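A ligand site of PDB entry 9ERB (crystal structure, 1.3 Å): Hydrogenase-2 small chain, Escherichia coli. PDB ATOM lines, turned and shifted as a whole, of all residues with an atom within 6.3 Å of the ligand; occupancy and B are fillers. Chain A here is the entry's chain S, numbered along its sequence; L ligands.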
ATOM      1  N   ILE A 190     -27.621 -16.252  -4.870  1.00  0.00           N
ATOM      2  CA  ILE A 190     -28.625 -15.935  -5.871  1.00  0.00           C
ATOM      3  C   ILE A 190     -28.145 -16.379  -7.243  1.00  0.00           C
ATOM      4  O   ILE A 190     -28.892 -16.976  -8.012  1.00  0.00           O
ATOM      5  CB  ILE A 190     -28.956 -14.422  -5.808  1.00  0.00           C
ATOM      6  CG1 ILE A 190     -29.761 -14.120  -4.534  1.00  0.00           C
ATOM      7  CG2 ILE A 190     -29.703 -13.988  -7.030  1.00  0.00           C
ATOM      8  CD1 ILE A 190     -29.929 -12.663  -4.206  1.00  0.00           C
ATOM      9  N   HIS A 191     -26.861 -16.166  -7.550  1.00  0.00           N
ATOM     10  CA  HIS A 191     -26.334 -16.569  -8.865  1.00  0.00           C
ATOM     11  C   HIS A 191     -26.318 -18.077  -9.061  1.00  0.00           C
ATOM     12  O   HIS A 191     -26.241 -18.512 -10.220  1.00  0.00           O
ATOM     13  CB  HIS A 191     -24.909 -15.993  -8.957  1.00  0.00           C
ATOM     14  CG  HIS A 191     -24.155 -16.256 -10.218  1.00  0.00           C
ATOM     15  ND1 HIS A 191     -24.339 -15.546 -11.387  1.00  0.00           N
ATOM     16  CD2 HIS A 191     -23.098 -17.084 -10.439  1.00  0.00           C
ATOM     17  CE1 HIS A 191     -23.460 -15.962 -12.291  1.00  0.00           C
ATOM     18  NE2 HIS A 191     -22.695 -16.884 -11.741  1.00  0.00           N
ATOM     19  N   GLU A 192     -26.338 -18.870  -7.980  1.00  0.00           N
ATOM     20  CA  GLU A 192     -26.396 -20.314  -8.112  1.00  0.00           C
ATOM     21  C   GLU A 192     -27.838 -20.815  -8.205  1.00  0.00           C
ATOM     22  O   GLU A 192     -28.078 -22.035  -8.177  1.00  0.00           O
ATOM     23  CB  GLU A 192     -25.611 -20.984  -6.991  1.00  0.00           C
ATOM     24  CG  GLU A 192     -24.107 -20.720  -7.095  1.00  0.00           C
ATOM     25  CD  GLU A 192     -23.505 -21.172  -8.408  1.00  0.00           C
ATOM     26  OE1 GLU A 192     -23.734 -22.326  -8.788  1.00  0.00           O
ATOM     27  OE2 GLU A 192     -22.875 -20.357  -9.130  1.00  0.00           O
ATOM     28  N   CYS A 194     -30.218 -18.586 -10.374  1.00  0.00           N
ATOM     29  CA  CYS A 194     -30.741 -17.449 -11.125  1.00  0.00           C
ATOM     30  C   CYS A 194     -31.089 -17.855 -12.555  1.00  0.00           C
ATOM     31  O   CYS A 194     -30.270 -18.495 -13.249  1.00  0.00           O
ATOM     32  CB  CYS A 194     -29.699 -16.323 -11.179  1.00  0.00           C
ATOM     33  SG  CYS A 194     -30.268 -14.880 -12.165  1.00  0.00           S
ATOM     34  N   GLU A 195     -32.274 -17.453 -13.002  1.00  0.00           N
ATOM     35  CA  GLU A 195     -32.758 -17.844 -14.325  1.00  0.00           C
ATOM     36  C   GLU A 195     -32.034 -17.155 -15.468  1.00  0.00           C
ATOM     37  O   GLU A 195     -32.228 -17.563 -16.627  1.00  0.00           O
ATOM     38  CB  GLU A 195     -34.254 -17.602 -14.449  1.00  0.00           C
ATOM     39  CG  GLU A 195     -34.718 -16.101 -14.434  1.00  0.00           C
ATOM     40  CD  GLU A 195     -34.854 -15.415 -13.080  1.00  0.00           C
ATOM     41  OE1 GLU A 195     -34.381 -15.931 -12.043  1.00  0.00           O
ATOM     42  OE2 GLU A 195     -35.498 -14.333 -13.085  1.00  0.00           O
ATOM     43  N   ARG A 196     -31.166 -16.168 -15.185  1.00  0.00           N
ATOM     44  CA  ARG A 196     -30.339 -15.573 -16.236  1.00  0.00           C
ATOM     45  C   ARG A 196     -28.978 -16.214 -16.318  1.00  0.00           C
ATOM     46  O   ARG A 196     -28.164 -15.792 -17.145  1.00  0.00           O
ATOM     47  CB  ARG A 196     -30.246 -14.065 -16.066  1.00  0.00           C
ATOM     48  CG  ARG A 196     -31.653 -13.470 -16.071  1.00  0.00           C
ATOM     49  CD  ARG A 196     -31.678 -11.982 -16.183  1.00  0.00           C
ATOM     50  NE  ARG A 196     -33.057 -11.508 -16.255  1.00  0.00           N
ATOM     51  CZ  ARG A 196     -33.423 -10.334 -16.716  1.00  0.00           C
ATOM     52  NH1 ARG A 196     -32.530  -9.465 -17.130  1.00  0.00           N
ATOM     53  NH2 ARG A 196     -34.706 -10.041 -16.769  1.00  0.00           N
ATOM     54  N   ARG A 197     -28.710 -17.258 -15.524  1.00  0.00           N
ATOM     55  CA  ARG A 197     -27.412 -17.926 -15.621  1.00  0.00           C
ATOM     56  C   ARG A 197     -27.122 -18.393 -17.045  1.00  0.00           C
ATOM     57  O   ARG A 197     -25.939 -18.339 -17.436  1.00  0.00           O
ATOM     58  CB  ARG A 197     -27.346 -19.091 -14.631  1.00  0.00           C
ATOM     59  CG  ARG A 197     -26.014 -19.844 -14.660  1.00  0.00           C
ATOM     60  CD  ARG A 197     -24.827 -18.975 -14.290  1.00  0.00           C
ATOM     61  NE  ARG A 197     -23.641 -19.797 -14.150  1.00  0.00           N
ATOM     62  CZ  ARG A 197     -23.287 -20.428 -13.039  1.00  0.00           C
ATOM     63  NH1 ARG A 197     -23.873 -20.185 -11.880  1.00  0.00           N
ATOM     64  NH2 ARG A 197     -22.332 -21.349 -13.103  1.00  0.00           N
ATOM     65  N   PRO A 198     -28.081 -18.904 -17.835  1.00  0.00           N
ATOM     66  CA  PRO A 198     -27.720 -19.313 -19.203  1.00  0.00           C
ATOM     67  C   PRO A 198     -27.083 -18.182 -19.985  1.00  0.00           C
ATOM     68  O   PRO A 198     -26.155 -18.420 -20.782  1.00  0.00           O
ATOM     69  CB  PRO A 198     -29.069 -19.685 -19.830  1.00  0.00           C
ATOM     70  CG  PRO A 198     -29.891 -20.149 -18.641  1.00  0.00           C
ATOM     71  CD  PRO A 198     -29.500 -19.189 -17.534  1.00  0.00           C
ATOM     72  N   PHE A 200     -25.423 -15.495 -18.708  1.00  0.00           N
ATOM     73  CA  PHE A 200     -24.079 -15.348 -18.154  1.00  0.00           C
ATOM     74  C   PHE A 200     -23.138 -16.347 -18.824  1.00  0.00           C
ATOM     75  O   PHE A 200     -22.049 -15.987 -19.287  1.00  0.00           O
ATOM     76  CB  PHE A 200     -24.163 -15.586 -16.644  1.00  0.00           C
ATOM     77  CG  PHE A 200     -22.855 -15.492 -15.920  1.00  0.00           C
ATOM     78  CD1 PHE A 200     -22.058 -16.612 -15.766  1.00  0.00           C
ATOM     79  CD2 PHE A 200     -22.427 -14.294 -15.366  1.00  0.00           C
ATOM     80  CE1 PHE A 200     -20.853 -16.545 -15.119  1.00  0.00           C
ATOM     81  CE2 PHE A 200     -21.220 -14.216 -14.684  1.00  0.00           C
ATOM     82  CZ  PHE A 200     -20.429 -15.357 -14.535  1.00  0.00           C
ATOM     83  N   PHE A 205     -24.874 -10.365 -22.267  1.00  0.00           N
ATOM     84  CA  PHE A 205     -24.912  -9.403 -21.177  1.00  0.00           C
ATOM     85  C   PHE A 205     -25.541  -8.100 -21.616  1.00  0.00           C
ATOM     86  O   PHE A 205     -25.191  -7.550 -22.665  1.00  0.00           O
ATOM     87  CB  PHE A 205     -23.499  -9.075 -20.700  1.00  0.00           C
ATOM     88  CG  PHE A 205     -22.740 -10.236 -20.102  1.00  0.00           C
ATOM     89  CD1 PHE A 205     -23.138 -10.781 -18.898  1.00  0.00           C
ATOM     90  CD2 PHE A 205     -21.564 -10.733 -20.700  1.00  0.00           C
ATOM     91  CE1 PHE A 205     -22.440 -11.804 -18.320  1.00  0.00           C
ATOM     92  CE2 PHE A 205     -20.871 -11.747 -20.113  1.00  0.00           C
ATOM     93  CZ  PHE A 205     -21.295 -12.305 -18.945  1.00  0.00           C
ATOM     94  N   TRP A 218     -31.301 -10.360 -20.795  1.00  0.00           N
ATOM     95  CA  TRP A 218     -29.991 -10.991 -20.624  1.00  0.00           C
ATOM     96  C   TRP A 218     -29.422 -10.750 -19.229  1.00  0.00           C
ATOM     97  O   TRP A 218     -29.992 -10.036 -18.395  1.00  0.00           O
ATOM     98  CB  TRP A 218     -29.045 -10.486 -21.713  1.00  0.00           C
ATOM     99  CG  TRP A 218     -29.308 -11.010 -23.095  1.00  0.00           C
ATOM    100  CD1 TRP A 218     -30.298 -11.835 -23.477  1.00  0.00           C
ATOM    101  CD2 TRP A 218     -28.542 -10.710 -24.286  1.00  0.00           C
ATOM    102  NE1 TRP A 218     -30.210 -12.086 -24.838  1.00  0.00           N
ATOM    103  CE2 TRP A 218     -29.149 -11.395 -25.344  1.00  0.00           C
ATOM    104  CE3 TRP A 218     -27.401  -9.951 -24.532  1.00  0.00           C
ATOM    105  CZ2 TRP A 218     -28.625 -11.363 -26.657  1.00  0.00           C
ATOM    106  CZ3 TRP A 218     -26.902  -9.899 -25.839  1.00  0.00           C
ATOM    107  CH2 TRP A 218     -27.516 -10.601 -26.871  1.00  0.00           C
ATOM    108  N   CYS A 219     -28.286 -11.402 -18.951  1.00  0.00           N
ATOM    109  CA  CYS A 219     -27.687 -11.327 -17.621  1.00  0.00           C
ATOM    110  C   CYS A 219     -27.216  -9.902 -17.340  1.00  0.00           C
ATOM    111  O   CYS A 219     -26.795  -9.180 -18.237  1.00  0.00           O
ATOM    112  CB  CYS A 219     -26.528 -12.323 -17.521  1.00  0.00           C
ATOM    113  SG  CYS A 219     -25.431 -12.137 -16.100  1.00  0.00           S
ATOM    114  N   LEU A 220     -27.339  -9.502 -16.061  1.00  0.00           N
ATOM    115  CA  LEU A 220     -27.018  -8.163 -15.573  1.00  0.00           C
ATOM    116  C   LEU A 220     -25.662  -8.052 -14.879  1.00  0.00           C
ATOM    117  O   LEU A 220     -25.386  -7.023 -14.216  1.00  0.00           O
ATOM    118  CB  LEU A 220     -28.169  -7.684 -14.663  1.00  0.00           C
ATOM    119  CG  LEU A 220     -29.559  -7.818 -15.240  1.00  0.00           C
ATOM    120  CD1 LEU A 220     -30.594  -7.156 -14.319  1.00  0.00           C
ATOM    121  CD2 LEU A 220     -29.678  -7.187 -16.602  1.00  0.00           C
ATOM    122  N   TYR A 221     -24.794  -9.069 -15.029  1.00  0.00           N
ATOM    123  CA  TYR A 221     -23.487  -9.048 -14.366  1.00  0.00           C
ATOM    124  C   TYR A 221     -22.725  -7.753 -14.626  1.00  0.00           C
ATOM    125  O   TYR A 221     -22.184  -7.131 -13.707  1.00  0.00           O
ATOM    126  CB  TYR A 221     -22.648 -10.260 -14.798  1.00  0.00           C
ATOM    127  CG  TYR A 221     -21.281 -10.216 -14.162  1.00  0.00           C
ATOM    128  CD1 TYR A 221     -21.115 -10.564 -12.841  1.00  0.00           C
ATOM    129  CD2 TYR A 221     -20.190  -9.732 -14.850  1.00  0.00           C
ATOM    130  CE1 TYR A 221     -19.898 -10.485 -12.199  1.00  0.00           C
ATOM    131  CE2 TYR A 221     -18.950  -9.623 -14.224  1.00  0.00           C
ATOM    132  CZ  TYR A 221     -18.821  -9.994 -12.905  1.00  0.00           C
ATOM    133  OH  TYR A 221     -17.583  -9.872 -12.294  1.00  0.00           O
ATOM    134  N   HIS A 222     -22.661  -7.352 -15.888  1.00  0.00           N
ATOM    135  CA  HIS A 222     -21.875  -6.177 -16.267  1.00  0.00           C
ATOM    136  C   HIS A 222     -22.568  -4.867 -15.953  1.00  0.00           C
ATOM    137  O   HIS A 222     -21.952  -3.812 -16.138  1.00  0.00           O
ATOM    138  CB  HIS A 222     -21.410  -6.275 -17.724  1.00  0.00           C
ATOM    139  CG  HIS A 222     -20.257  -7.205 -17.871  1.00  0.00           C
ATOM    140  ND1 HIS A 222     -18.992  -6.889 -17.415  1.00  0.00           N
ATOM    141  CD2 HIS A 222     -20.179  -8.463 -18.361  1.00  0.00           C
ATOM    142  CE1 HIS A 222     -18.193  -7.921 -17.609  1.00  0.00           C
ATOM    143  NE2 HIS A 222     -18.887  -8.887 -18.184  1.00  0.00           N
ATOM    144  N   CYS A 225     -24.452  -6.666 -11.124  1.00  0.00           N
ATOM    145  CA  CYS A 225     -25.221  -7.615 -10.343  1.00  0.00           C
ATOM    146  C   CYS A 225     -24.362  -8.291  -9.288  1.00  0.00           C
ATOM    147  O   CYS A 225     -23.318  -8.873  -9.587  1.00  0.00           O
ATOM    148  CB  CYS A 225     -25.832  -8.666 -11.264  1.00  0.00           C
ATOM    149  SG  CYS A 225     -26.991  -9.767 -10.397  1.00  0.00           S
ATOM    150  N   LYS A 226     -24.856  -8.273  -8.054  1.00  0.00           N
ATOM    151  CA  LYS A 226     -24.174  -8.863  -6.906  1.00  0.00           C
ATOM    152  C   LYS A 226     -24.653 -10.272  -6.578  1.00  0.00           C
ATOM    153  O   LYS A 226     -24.258 -10.834  -5.558  1.00  0.00           O
ATOM    154  CB  LYS A 226     -24.270  -7.955  -5.683  1.00  0.00           C
ATOM    155  CG  LYS A 226     -23.747  -6.521  -5.916  1.00  0.00           C
ATOM    156  CD  LYS A 226     -22.339  -6.493  -6.501  1.00  0.00           C
ATOM    157  CE  LYS A 226     -21.724  -5.122  -6.521  1.00  0.00           C
ATOM    158  NZ  LYS A 226     -22.618  -4.110  -7.178  1.00  0.00           N
ATOM    159  N   GLY A 227     -25.514 -10.850  -7.423  1.00  0.00           N
ATOM    160  CA  GLY A 227     -25.941 -12.227  -7.231  1.00  0.00           C
ATOM    161  C   GLY A 227     -24.818 -13.211  -6.972  1.00  0.00           C
ATOM    162  O   GLY A 227     -24.992 -14.123  -6.147  1.00  0.00           O
ATOM    163  N   PRO A 228     -23.654 -13.059  -7.608  1.00  0.00           N
ATOM    164  CA  PRO A 228     -22.560 -14.005  -7.366  1.00  0.00           C
ATOM    165  C   PRO A 228     -22.009 -14.000  -5.971  1.00  0.00           C
ATOM    166  O   PRO A 228     -21.275 -14.941  -5.618  1.00  0.00           O
ATOM    167  CB  PRO A 228     -21.497 -13.647  -8.422  1.00  0.00           C
ATOM    168  CG  PRO A 228     -22.252 -12.942  -9.503  1.00  0.00           C
ATOM    169  CD  PRO A 228     -23.429 -12.238  -8.807  1.00  0.00           C
ATOM    170  N   TRP A 246     -38.760  -9.702  -9.006  1.00  0.00           N
ATOM    171  CA  TRP A 246     -37.589  -9.435  -8.184  1.00  0.00           C
ATOM    172  C   TRP A 246     -36.722  -8.475  -8.967  1.00  0.00           C
ATOM    173  O   TRP A 246     -36.985  -8.223 -10.148  1.00  0.00           O
ATOM    174  CB  TRP A 246     -36.852 -10.719  -7.794  1.00  0.00           C
ATOM    175  CG  TRP A 246     -36.086 -11.502  -8.854  1.00  0.00           C
ATOM    176  CD1 TRP A 246     -36.618 -12.263  -9.893  1.00  0.00           C
ATOM    177  CD2 TRP A 246     -34.653 -11.730  -8.882  1.00  0.00           C
ATOM    178  NE1 TRP A 246     -35.589 -12.921 -10.547  1.00  0.00           N
ATOM    179  CE2 TRP A 246     -34.390 -12.593  -9.967  1.00  0.00           C
ATOM    180  CE3 TRP A 246     -33.583 -11.296  -8.091  1.00  0.00           C
ATOM    181  CZ2 TRP A 246     -33.101 -13.037 -10.254  1.00  0.00           C
ATOM    182  CZ3 TRP A 246     -32.330 -11.742  -8.390  1.00  0.00           C
ATOM    183  CH2 TRP A 246     -32.094 -12.606  -9.459  1.00  0.00           C
ATOM    184  N   VAL A 248     -33.785  -8.316 -10.485  1.00  0.00           N
ATOM    185  CA  VAL A 248     -33.185  -8.727 -11.763  1.00  0.00           C
ATOM    186  C   VAL A 248     -34.267  -8.964 -12.807  1.00  0.00           C
ATOM    187  O   VAL A 248     -34.138  -8.555 -13.964  1.00  0.00           O
ATOM    188  CB  VAL A 248     -32.307  -9.969 -11.538  1.00  0.00           C
ATOM    189  CG1 VAL A 248     -31.969 -10.676 -12.841  1.00  0.00           C
ATOM    190  CG2 VAL A 248     -31.026  -9.545 -10.819  1.00  0.00           C
ATOM    191  N   PRO A 253     -29.753  -4.865 -11.636  1.00  0.00           N
ATOM    192  CA  PRO A 253     -28.886  -5.822 -10.929  1.00  0.00           C
ATOM    193  C   PRO A 253     -29.273  -5.938  -9.453  1.00  0.00           C
ATOM    194  O   PRO A 253     -29.746  -4.984  -8.821  1.00  0.00           O
ATOM    195  CB  PRO A 253     -27.488  -5.211 -11.067  1.00  0.00           C
ATOM    196  CG  PRO A 253     -27.714  -3.748 -11.442  1.00  0.00           C
ATOM    197  CD  PRO A 253     -28.995  -3.745 -12.218  1.00  0.00           C
ATOM    198  N   CYS A 254     -28.999  -7.114  -8.905  1.00  0.00           N
ATOM    199  CA  CYS A 254     -28.925  -7.228  -7.452  1.00  0.00           C
ATOM    200  C   CYS A 254     -27.826  -6.327  -6.938  1.00  0.00           C
ATOM    201  O   CYS A 254     -26.760  -6.220  -7.548  1.00  0.00           O
ATOM    202  CB  CYS A 254     -28.597  -8.678  -7.065  1.00  0.00           C
ATOM    203  SG  CYS A 254     -28.318  -9.015  -5.298  1.00  0.00           S
HETATM  204 FE1  LIG L   1     -26.423 -12.761 -14.144  1.00  0.00          FE
HETATM  205 FE2  LIG L   1     -26.878 -11.651 -11.651  1.00  0.00          FE
HETATM  206 FE3  LIG L   1     -25.701 -14.124 -11.905  1.00  0.00          FE
HETATM  207 FE4  LIG L   1     -28.315 -13.827 -12.504  1.00  0.00          FE
HETATM  208  S1  LIG L   1     -27.313 -13.533 -10.437  1.00  0.00           S
HETATM  209  S2  LIG L   1     -26.796 -14.955 -13.759  1.00  0.00           S
HETATM  210  S3  LIG L   1     -28.321 -11.721 -13.462  1.00  0.00           S
HETATM  211  S4  LIG L   1     -24.831 -12.129 -12.556  1.00  0.00           S
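ND1 of His 191 is bound to FE3 of the ligand. FE4 of the ligand is bound by SG of Cys 194 (2.2 Å). FE2 of the ligand is bound by SG of Cys 225 (2.3 Å). The side-chain sulfur (SG) of Cys 219 binds an iron atom (FE1) of the ligand (2.3 Å). The backbone NH (N) of Arg 197 lies close to a sulfur (S2) of the ligand, at 3.5 Å. A sulfur (S3) of the ligand sits close to the backbone NH (N) of Leu 220.
The backbone carbonyl oxygen (O) of His 191 is in hydrogen-bond range of the guanidinium group (NH1) of Arg 197 (3.3 Å). The backbone carbonyl oxygen (O) of Gly 227 sits at hydrogen-bond distance from the backbone NH (N) of His 191, at 3.1 Å. The side-chain sulfur (SG) of Cys 194 sits close to the backbone NH (N) of Arg 196 (3.4 Å). N of Gly 227 lies close to SG of Cys 225. SG of Cys 219 lies close to N of Tyr 221. The guanidinium group (NH1) of Arg 197 is in salt-bridge range of the side-chain carboxylate (OE2) of Glu 192. The backbone carbonyl oxygen (O) of Val 248 sits at hydrogen-bond distance from the guanidinium group (NH2) of Arg 196, at 3.2 Å. The guanidinium group of Arg 196 is in hydrogen-bond range of the backbone carbonyl oxygen of Trp 218 (2.9 Å).
O of Arg 196 sits close to S2 of the ligand (3.7 Å). Phe 200 touches the ligand (CB to S2, 3.96 Å). CB of Tyr 221 touches S4 of the ligand, 3.6 Å away. Gly 227 touches the ligand (CA to S1, 3.7 Å). Val 248 touches the ligand. Hydrophobic or aromatic side chains that line the ligand: His 191, Phe 200, Tyr 221 and Val 248.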
